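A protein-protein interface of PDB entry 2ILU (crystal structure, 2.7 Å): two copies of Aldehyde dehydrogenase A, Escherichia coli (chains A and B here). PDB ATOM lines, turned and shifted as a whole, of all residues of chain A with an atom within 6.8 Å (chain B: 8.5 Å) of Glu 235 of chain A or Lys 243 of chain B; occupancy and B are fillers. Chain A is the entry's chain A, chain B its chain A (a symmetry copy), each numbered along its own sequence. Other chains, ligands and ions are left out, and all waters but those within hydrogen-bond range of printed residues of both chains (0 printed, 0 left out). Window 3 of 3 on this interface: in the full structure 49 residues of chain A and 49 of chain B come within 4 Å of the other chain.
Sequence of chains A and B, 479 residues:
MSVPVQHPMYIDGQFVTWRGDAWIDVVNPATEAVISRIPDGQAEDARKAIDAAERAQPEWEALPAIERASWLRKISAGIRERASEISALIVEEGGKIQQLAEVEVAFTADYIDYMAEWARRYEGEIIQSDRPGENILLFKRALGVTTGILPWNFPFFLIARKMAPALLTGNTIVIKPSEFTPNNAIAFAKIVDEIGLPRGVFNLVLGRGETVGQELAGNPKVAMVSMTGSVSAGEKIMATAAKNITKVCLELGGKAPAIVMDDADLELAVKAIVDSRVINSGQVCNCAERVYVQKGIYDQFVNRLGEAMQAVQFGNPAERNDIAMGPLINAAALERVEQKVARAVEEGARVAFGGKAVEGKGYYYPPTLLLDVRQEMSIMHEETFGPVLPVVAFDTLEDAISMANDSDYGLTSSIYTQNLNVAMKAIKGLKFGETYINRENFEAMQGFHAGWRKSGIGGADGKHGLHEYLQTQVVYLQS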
ATOM      1  N   MET A 227       2.612  16.558   4.751  1.00  0.00           N
ATOM      2  CA  MET A 227       1.221  16.430   5.136  1.00  0.00           C
ATOM      3  C   MET A 227       0.885  15.161   5.927  1.00  0.00           C
ATOM      4  O   MET A 227       1.491  14.116   5.704  1.00  0.00           O
ATOM      5  CB  MET A 227       0.331  16.517   3.893  1.00  0.00           C
ATOM      6  CG  MET A 227      -1.135  16.178   4.128  1.00  0.00           C
ATOM      7  SD  MET A 227      -1.474  14.421   3.934  1.00  0.00           S
ATOM      8  CE  MET A 227      -3.110  14.294   4.535  1.00  0.00           C
ATOM      9  N   SER A 230      -5.304  11.330   5.650  1.00  0.00           N
ATOM     10  CA  SER A 230      -5.821  10.153   4.951  1.00  0.00           C
ATOM     11  C   SER A 230      -5.099   9.799   3.639  1.00  0.00           C
ATOM     12  O   SER A 230      -4.623  10.701   2.966  1.00  0.00           O
ATOM     13  CB  SER A 230      -7.303  10.351   4.624  1.00  0.00           C
ATOM     14  OG  SER A 230      -7.453  11.181   3.475  1.00  0.00           O
ATOM     15  N   VAL A 231      -5.044   8.519   3.294  1.00  0.00           N
ATOM     16  CA  VAL A 231      -4.401   8.110   2.052  1.00  0.00           C
ATOM     17  C   VAL A 231      -4.925   8.922   0.842  1.00  0.00           C
ATOM     18  O   VAL A 231      -4.138   9.320  -0.021  1.00  0.00           O
ATOM     19  CB  VAL A 231      -4.631   6.602   1.780  1.00  0.00           C
ATOM     20  CG1 VAL A 231      -6.120   6.322   1.639  1.00  0.00           C
ATOM     21  CG2 VAL A 231      -3.897   6.175   0.527  1.00  0.00           C
ATOM     22  N   SER A 232      -6.231   9.161   0.818  1.00  0.00           N
ATOM     23  CA  SER A 232      -6.871   9.924  -0.245  1.00  0.00           C
ATOM     24  C   SER A 232      -6.252  11.321  -0.442  1.00  0.00           C
ATOM     25  O   SER A 232      -5.912  11.687  -1.571  1.00  0.00           O
ATOM     26  CB  SER A 232      -8.361  10.063   0.062  1.00  0.00           C
ATOM     27  OG  SER A 232      -8.992  10.934  -0.856  1.00  0.00           O
ATOM     28  N   ALA A 233      -6.128  12.079   0.641  1.00  0.00           N
ATOM     29  CA  ALA A 233      -5.524  13.397   0.554  1.00  0.00           C
ATOM     30  C   ALA A 233      -4.038  13.309   0.156  1.00  0.00           C
ATOM     31  O   ALA A 233      -3.550  14.155  -0.596  1.00  0.00           O
ATOM     32  CB  ALA A 233      -5.669  14.124   1.891  1.00  0.00           C
ATOM     33  N   GLY A 234      -3.357  12.286   0.662  1.00  0.00           N
ATOM     34  CA  GLY A 234      -1.958  12.102   0.336  1.00  0.00           C
ATOM     35  C   GLY A 234      -1.836  11.895  -1.157  1.00  0.00           C
ATOM     36  O   GLY A 234      -0.898  12.385  -1.786  1.00  0.00           O
ATOM     37  N   GLU A 235      -2.786  11.165  -1.730  1.00  0.00           N
ATOM     38  CA  GLU A 235      -2.764  10.920  -3.158  1.00  0.00           C
ATOM     39  C   GLU A 235      -2.948  12.218  -3.978  1.00  0.00           C
ATOM     40  O   GLU A 235      -2.284  12.392  -4.999  1.00  0.00           O
ATOM     41  CB  GLU A 235      -3.853   9.921  -3.529  1.00  0.00           C
ATOM     42  CG  GLU A 235      -3.663   9.290  -4.898  1.00  0.00           C
ATOM     43  CD  GLU A 235      -4.818   8.374  -5.289  1.00  0.00           C
ATOM     44  OE1 GLU A 235      -5.264   7.570  -4.429  1.00  0.00           O
ATOM     45  OE2 GLU A 235      -5.272   8.458  -6.457  1.00  0.00           O
ATOM     46  N   LYS A 236      -3.830  13.101  -3.528  1.00  0.00           N
ATOM     47  CA  LYS A 236      -4.045  14.352  -4.232  1.00  0.00           C
ATOM     48  C   LYS A 236      -2.864  15.297  -4.047  1.00  0.00           C
ATOM     49  O   LYS A 236      -2.517  16.033  -4.974  1.00  0.00           O
ATOM     50  CB  LYS A 236      -5.333  15.019  -3.751  1.00  0.00           C
ATOM     51  CG  LYS A 236      -6.578  14.201  -4.046  1.00  0.00           C
ATOM     52  CD  LYS A 236      -7.843  14.867  -3.514  1.00  0.00           C
ATOM     53  CE  LYS A 236      -9.095  14.064  -3.861  1.00  0.00           C
ATOM     54  NZ  LYS A 236      -9.048  12.697  -3.282  1.00  0.00           N
ATOM     55  N   ILE A 237      -2.260  15.265  -2.866  1.00  0.00           N
ATOM     56  CA  ILE A 237      -1.105  16.098  -2.609  1.00  0.00           C
ATOM     57  C   ILE A 237       0.124  15.639  -3.411  1.00  0.00           C
ATOM     58  O   ILE A 237       0.787  16.479  -4.018  1.00  0.00           O
ATOM     59  CB  ILE A 237      -0.767  16.115  -1.109  1.00  0.00           C
ATOM     60  CG1 ILE A 237      -1.887  16.835  -0.356  1.00  0.00           C
ATOM     61  CG2 ILE A 237       0.578  16.793  -0.871  1.00  0.00           C
ATOM     62  CD1 ILE A 237      -1.739  16.821   1.135  1.00  0.00           C
ATOM     63  N   MET A 238       0.409  14.339  -3.420  1.00  0.00           N
ATOM     64  CA  MET A 238       1.545  13.861  -4.191  1.00  0.00           C
ATOM     65  C   MET A 238       1.341  14.088  -5.687  1.00  0.00           C
ATOM     66  O   MET A 238       2.269  14.523  -6.365  1.00  0.00           O
ATOM     67  CB  MET A 238       1.806  12.379  -3.935  1.00  0.00           C
ATOM     68  CG  MET A 238       3.137  11.898  -4.504  1.00  0.00           C
ATOM     69  SD  MET A 238       3.592  10.256  -3.916  1.00  0.00           S
ATOM     70  CE  MET A 238       4.683   9.715  -5.258  1.00  0.00           C
ATOM     71  N   ALA A 239       0.139  13.814  -6.179  1.00  0.00           N
ATOM     72  CA  ALA A 239      -0.134  14.033  -7.587  1.00  0.00           C
ATOM     73  C   ALA A 239       0.115  15.509  -8.000  1.00  0.00           C
ATOM     74  O   ALA A 239       0.689  15.742  -9.061  1.00  0.00           O
ATOM     75  CB  ALA A 239      -1.561  13.621  -7.908  1.00  0.00           C
ATOM     76  N   THR A 240      -0.306  16.460  -7.165  1.00  0.00           N
ATOM     77  CA  THR A 240      -0.099  17.876  -7.450  1.00  0.00           C
ATOM     78  C   THR A 240       1.377  18.280  -7.345  1.00  0.00           C
ATOM     79  O   THR A 240       1.869  19.045  -8.188  1.00  0.00           O
ATOM     80  CB  THR A 240      -0.911  18.757  -6.494  1.00  0.00           C
ATOM     81  OG1 THR A 240      -2.305  18.520  -6.706  1.00  0.00           O
ATOM     82  CG2 THR A 240      -0.616  20.230  -6.739  1.00  0.00           C
ATOM     83  N   LEU A 250       4.744  12.480   3.522  1.00  0.00           N
ATOM     84  CA  LEU A 250       3.405  12.052   3.914  1.00  0.00           C
ATOM     85  C   LEU A 250       3.324  11.011   5.045  1.00  0.00           C
ATOM     86  O   LEU A 250       4.167  10.127   5.144  1.00  0.00           O
ATOM     87  CB  LEU A 250       2.665  11.497   2.691  1.00  0.00           C
ATOM     88  CG  LEU A 250       2.837  12.351   1.429  1.00  0.00           C
ATOM     89  CD1 LEU A 250       2.221  11.676   0.232  1.00  0.00           C
ATOM     90  CD2 LEU A 250       2.209  13.713   1.653  1.00  0.00           C
ATOM     91  N   LEU A 252       0.101   8.924   6.257  1.00  0.00           N
ATOM     92  CA  LEU A 252      -1.309   8.606   6.084  1.00  0.00           C
ATOM     93  C   LEU A 252      -1.858   7.514   7.036  1.00  0.00           C
ATOM     94  O   LEU A 252      -2.808   6.806   6.688  1.00  0.00           O
ATOM     95  CB  LEU A 252      -1.541   8.235   4.613  1.00  0.00           C
ATOM     96  CG  LEU A 252      -0.690   9.115   3.676  1.00  0.00           C
ATOM     97  CD1 LEU A 252      -0.915   8.756   2.229  1.00  0.00           C
ATOM     98  CD2 LEU A 252      -1.026  10.567   3.906  1.00  0.00           C
ATOM     99  N   LYS A 454       1.386   2.140   1.461  1.00  0.00           N
ATOM    100  CA  LYS A 454       0.585   3.357   1.378  1.00  0.00           C
ATOM    101  C   LYS A 454       0.574   4.223   2.671  1.00  0.00           C
ATOM    102  O   LYS A 454      -0.040   5.293   2.682  1.00  0.00           O
ATOM    103  CB  LYS A 454      -0.854   3.015   0.979  1.00  0.00           C
ATOM    104  CG  LYS A 454      -1.000   2.441  -0.427  1.00  0.00           C
ATOM    105  CD  LYS A 454      -2.468   2.244  -0.784  1.00  0.00           C
ATOM    106  CE  LYS A 454      -2.646   1.689  -2.189  1.00  0.00           C
ATOM    107  NZ  LYS A 454      -4.086   1.609  -2.584  1.00  0.00           N
ATOM    108  N   GLN B 214       4.648   3.320 -17.700  1.00  0.00           N
ATOM    109  CA  GLN B 214       3.550   3.670 -16.813  1.00  0.00           C
ATOM    110  C   GLN B 214       3.169   2.520 -15.890  1.00  0.00           C
ATOM    111  O   GLN B 214       2.794   2.761 -14.745  1.00  0.00           O
ATOM    112  CB  GLN B 214       2.336   4.120 -17.616  1.00  0.00           C
ATOM    113  CG  GLN B 214       2.460   5.547 -18.119  1.00  0.00           C
ATOM    114  CD  GLN B 214       2.513   6.565 -16.985  1.00  0.00           C
ATOM    115  OE1 GLN B 214       1.560   6.708 -16.219  1.00  0.00           O
ATOM    116  NE2 GLN B 214       3.628   7.271 -16.876  1.00  0.00           N
ATOM    117  N   ALA B 217       5.459   2.137 -12.981  1.00  0.00           N
ATOM    118  CA  ALA B 217       5.266   3.181 -11.984  1.00  0.00           C
ATOM    119  C   ALA B 217       3.916   3.128 -11.250  1.00  0.00           C
ATOM    120  O   ALA B 217       3.865   3.470 -10.068  1.00  0.00           O
ATOM    121  CB  ALA B 217       5.432   4.556 -12.636  1.00  0.00           C
ATOM    122  N   GLY B 218       2.864   2.701 -11.944  1.00  0.00           N
ATOM    123  CA  GLY B 218       1.543   2.663 -11.346  1.00  0.00           C
ATOM    124  C   GLY B 218       1.106   1.361 -10.725  1.00  0.00           C
ATOM    125  O   GLY B 218       0.028   1.291 -10.148  1.00  0.00           O
ATOM    126  N   ASN B 219       1.925   0.325 -10.835  1.00  0.00           N
ATOM    127  CA  ASN B 219       1.568  -0.960 -10.255  1.00  0.00           C
ATOM    128  C   ASN B 219       1.636  -0.982  -8.705  1.00  0.00           C
ATOM    129  O   ASN B 219       2.689  -0.718  -8.125  1.00  0.00           O
ATOM    130  CB  ASN B 219       2.463  -2.048 -10.846  1.00  0.00           C
ATOM    131  CG  ASN B 219       1.960  -3.447 -10.546  1.00  0.00           C
ATOM    132  OD1 ASN B 219       1.892  -3.856  -9.387  1.00  0.00           O
ATOM    133  ND2 ASN B 219       1.599  -4.187 -11.593  1.00  0.00           N
ATOM    134  N   PRO B 220       0.521  -1.298  -8.042  1.00  0.00           N
ATOM    135  CA  PRO B 220       0.474  -1.342  -6.576  1.00  0.00           C
ATOM    136  C   PRO B 220       1.537  -2.236  -5.897  1.00  0.00           C
ATOM    137  O   PRO B 220       1.829  -2.026  -4.724  1.00  0.00           O
ATOM    138  CB  PRO B 220      -0.955  -1.815  -6.290  1.00  0.00           C
ATOM    139  CG  PRO B 220      -1.286  -2.663  -7.493  1.00  0.00           C
ATOM    140  CD  PRO B 220      -0.719  -1.839  -8.630  1.00  0.00           C
ATOM    141  N   LYS B 236       5.222  12.633 -15.281  1.00  0.00           N
ATOM    142  CA  LYS B 236       4.218  11.615 -15.526  1.00  0.00           C
ATOM    143  C   LYS B 236       4.431  10.403 -14.627  1.00  0.00           C
ATOM    144  O   LYS B 236       3.457   9.787 -14.186  1.00  0.00           O
ATOM    145  CB  LYS B 236       4.237  11.190 -16.994  1.00  0.00           C
ATOM    146  CG  LYS B 236       3.876  12.314 -17.948  1.00  0.00           C
ATOM    147  CD  LYS B 236       3.949  11.876 -19.407  1.00  0.00           C
ATOM    148  CE  LYS B 236       3.534  12.997 -20.357  1.00  0.00           C
ATOM    149  NZ  LYS B 236       4.409  14.188 -20.219  1.00  0.00           N
ATOM    150  N   ILE B 237       5.689  10.080 -14.358  1.00  0.00           N
ATOM    151  CA  ILE B 237       5.993   8.969 -13.482  1.00  0.00           C
ATOM    152  C   ILE B 237       5.607   9.267 -12.024  1.00  0.00           C
ATOM    153  O   ILE B 237       4.981   8.420 -11.387  1.00  0.00           O
ATOM    154  CB  ILE B 237       7.484   8.603 -13.559  1.00  0.00           C
ATOM    155  CG1 ILE B 237       7.786   8.039 -14.948  1.00  0.00           C
ATOM    156  CG2 ILE B 237       7.845   7.600 -12.469  1.00  0.00           C
ATOM    157  CD1 ILE B 237       9.234   7.749 -15.197  1.00  0.00           C
ATOM    158  N   MET B 238       5.963  10.445 -11.516  1.00  0.00           N
ATOM    159  CA  MET B 238       5.591  10.777 -10.150  1.00  0.00           C
ATOM    160  C   MET B 238       4.076  10.877  -9.992  1.00  0.00           C
ATOM    161  O   MET B 238       3.535  10.369  -9.012  1.00  0.00           O
ATOM    162  CB  MET B 238       6.236  12.086  -9.702  1.00  0.00           C
ATOM    163  CG  MET B 238       6.099  12.339  -8.204  1.00  0.00           C
ATOM    164  SD  MET B 238       7.138  13.696  -7.630  1.00  0.00           S
ATOM    165  CE  MET B 238       6.230  14.202  -6.146  1.00  0.00           C
ATOM    166  N   ALA B 239       3.411  11.508 -10.951  1.00  0.00           N
ATOM    167  CA  ALA B 239       1.967  11.616 -10.880  1.00  0.00           C
ATOM    168  C   ALA B 239       1.286  10.223 -10.802  1.00  0.00           C
ATOM    169  O   ALA B 239       0.352  10.059 -10.021  1.00  0.00           O
ATOM    170  CB  ALA B 239       1.446  12.400 -12.074  1.00  0.00           C
ATOM    171  N   THR B 240       1.764   9.261 -11.593  1.00  0.00           N
ATOM    172  CA  THR B 240       1.211   7.912 -11.578  1.00  0.00           C
ATOM    173  C   THR B 240       1.538   7.164 -10.279  1.00  0.00           C
ATOM    174  O   THR B 240       0.669   6.470  -9.730  1.00  0.00           O
ATOM    175  CB  THR B 240       1.734   7.086 -12.757  1.00  0.00           C
ATOM    176  OG1 THR B 240       1.284   7.674 -13.981  1.00  0.00           O
ATOM    177  CG2 THR B 240       1.224   5.654 -12.680  1.00  0.00           C
ATOM    178  N   ALA B 241       2.778   7.299  -9.818  1.00  0.00           N
ATOM    179  CA  ALA B 241       3.185   6.676  -8.573  1.00  0.00           C
ATOM    180  C   ALA B 241       2.321   7.185  -7.406  1.00  0.00           C
ATOM    181  O   ALA B 241       2.107   6.455  -6.444  1.00  0.00           O
ATOM    182  CB  ALA B 241       4.659   6.975  -8.299  1.00  0.00           C
ATOM    183  N   ALA B 242       1.852   8.424  -7.525  1.00  0.00           N
ATOM    184  CA  ALA B 242       1.007   9.054  -6.518  1.00  0.00           C
ATOM    185  C   ALA B 242      -0.232   8.227  -6.179  1.00  0.00           C
ATOM    186  O   ALA B 242      -0.633   8.180  -5.018  1.00  0.00           O
ATOM    187  CB  ALA B 242       0.583  10.444  -6.990  1.00  0.00           C
ATOM    188  N   LYS B 243      -0.819   7.599  -7.187  1.00  0.00           N
ATOM    189  CA  LYS B 243      -1.997   6.777  -6.984  1.00  0.00           C
ATOM    190  C   LYS B 243      -1.843   5.746  -5.853  1.00  0.00           C
ATOM    191  O   LYS B 243      -2.794   5.520  -5.113  1.00  0.00           O
ATOM    192  CB  LYS B 243      -2.353   6.074  -8.294  1.00  0.00           C
ATOM    193  CG  LYS B 243      -2.848   7.038  -9.351  1.00  0.00           C
ATOM    194  CD  LYS B 243      -2.923   6.407 -10.732  1.00  0.00           C
ATOM    195  CE  LYS B 243      -3.535   7.388 -11.745  1.00  0.00           C
ATOM    196  NZ  LYS B 243      -2.816   8.698 -11.833  1.00  0.00           N
ATOM    197  N   ASN B 244      -0.665   5.153  -5.729  1.00  0.00           N
ATOM    198  CA  ASN B 244      -0.438   4.171  -4.687  1.00  0.00           C
ATOM    199  C   ASN B 244       0.579   4.625  -3.643  1.00  0.00           C
ATOM    200  O   ASN B 244       1.153   3.782  -2.945  1.00  0.00           O
ATOM    201  CB  ASN B 244       0.038   2.869  -5.310  1.00  0.00           C
ATOM    202  CG  ASN B 244      -0.871   2.399  -6.411  1.00  0.00           C
ATOM    203  OD1 ASN B 244      -2.051   2.138  -6.189  1.00  0.00           O
ATOM    204  ND2 ASN B 244      -0.329   2.293  -7.611  1.00  0.00           N
ATOM    205  N   ILE B 245       0.776   5.932  -3.533  1.00  0.00           N
ATOM    206  CA  ILE B 245       1.755   6.447  -2.603  1.00  0.00           C
ATOM    207  C   ILE B 245       3.082   5.705  -2.786  1.00  0.00           C
ATOM    208  O   ILE B 245       3.793   5.427  -1.828  1.00  0.00           O
ATOM    209  CB  ILE B 245       1.270   6.304  -1.154  1.00  0.00           C
ATOM    210  CG1 ILE B 245      -0.179   6.766  -1.057  1.00  0.00           C
ATOM    211  CG2 ILE B 245       2.128   7.159  -0.233  1.00  0.00           C
ATOM    212  CD1 ILE B 245      -0.400   8.177  -1.572  1.00  0.00           C
ATOM    213  N   THR B 246       3.373   5.374  -4.032  1.00  0.00           N
ATOM    214  CA  THR B 246       4.600   4.681  -4.350  1.00  0.00           C
ATOM    215  C   THR B 246       5.836   5.605  -4.292  1.00  0.00           C
ATOM    216  O   THR B 246       5.798   6.730  -4.794  1.00  0.00           O
ATOM    217  CB  THR B 246       4.492   4.023  -5.743  1.00  0.00           C
ATOM    218  OG1 THR B 246       3.484   3.004  -5.695  1.00  0.00           O
ATOM    219  CG2 THR B 246       5.820   3.406  -6.165  1.00  0.00           C
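Met 238 of chain A touches its own counterpart, Met 238 of chain B.
Among the printed residues, merely in contact across the chains: Glu 235 of chain A with Ala 242 of chain B (3.2 Å), Glu 235 of chain A with Ile 245 of chain B (3.8 Å), Met 238 of chain A with Met 238 of chain B (3.98 Å), Met 238 of chain A with Ala 242 of chain B (3.8 Å), Met 238 of chain A with Thr 246 of chain B (3.2 Å), Ala 239 of chain A with Ala 242 of chain B (3.5 Å), Leu 252 of chain A with Ile 245 of chain B (3.9 Å), Lys 454 of chain A with Asn 244 of chain B (3.6 Å) and Lys 454 of chain A with Ile 245 of chain B (3.9 Å).
Printed residues of chain B within 4 Å of Glu 235 of chain A: Ala 242 (3.2 Å), Lys 243 (3.3 Å) and Ile 245 (3.8 Å). Of chain A, only Glu 235 comes within 4 Å of Lys 243 of chain B. Printed residues of chain A within 4 Å of Met 238 of chain B: Met 238 (3.98 Å). Of the printed residues of chain A, Asn 244 of chain B touches Lys 454 (3.6 Å). Printed residues of chain B within 4 Å of Ala 239 of chain A: Ala 242 (3.5 Å). Of the printed residues of chain B, Met 238 of chain A touches Met 238, Ala 242 and Thr 246. Of the printed residues of chain B, Lys 454 of chain A touches Asn 244 (3.6 Å) and Ile 245 (3.9 Å). Ala 239 of chain B touches none of the printed residues of chain A.
The side-chain carboxylate of Glu 235 of chain A lies close to the backbone carbonyl oxygen of Lys 243 of chain B (3.3 Å).
Printed residues of chain B that touch a printed residue of chain A: Met 238, Ala 242, Lys 243, Asn 244, Ile 245 and Thr 246. Hydrophobic or aromatic side chains of chain B that line the printed part of chain A: Met 238, Ala 242 and Ile 245. Printed residues of chain A that touch a printed residue of chain B: Glu 235, Met 238, Ala 239, Leu 252 and Lys 454.
O of Gly 218 of chain B is in hydrogen-bond range of ND2 of Asn 244 of chain B (2.8 Å). The backbone carbonyl oxygen of Ala 241 of chain B is in hydrogen-bond range of the backbone NH of Thr 246 of chain B, 2.9 Å away.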
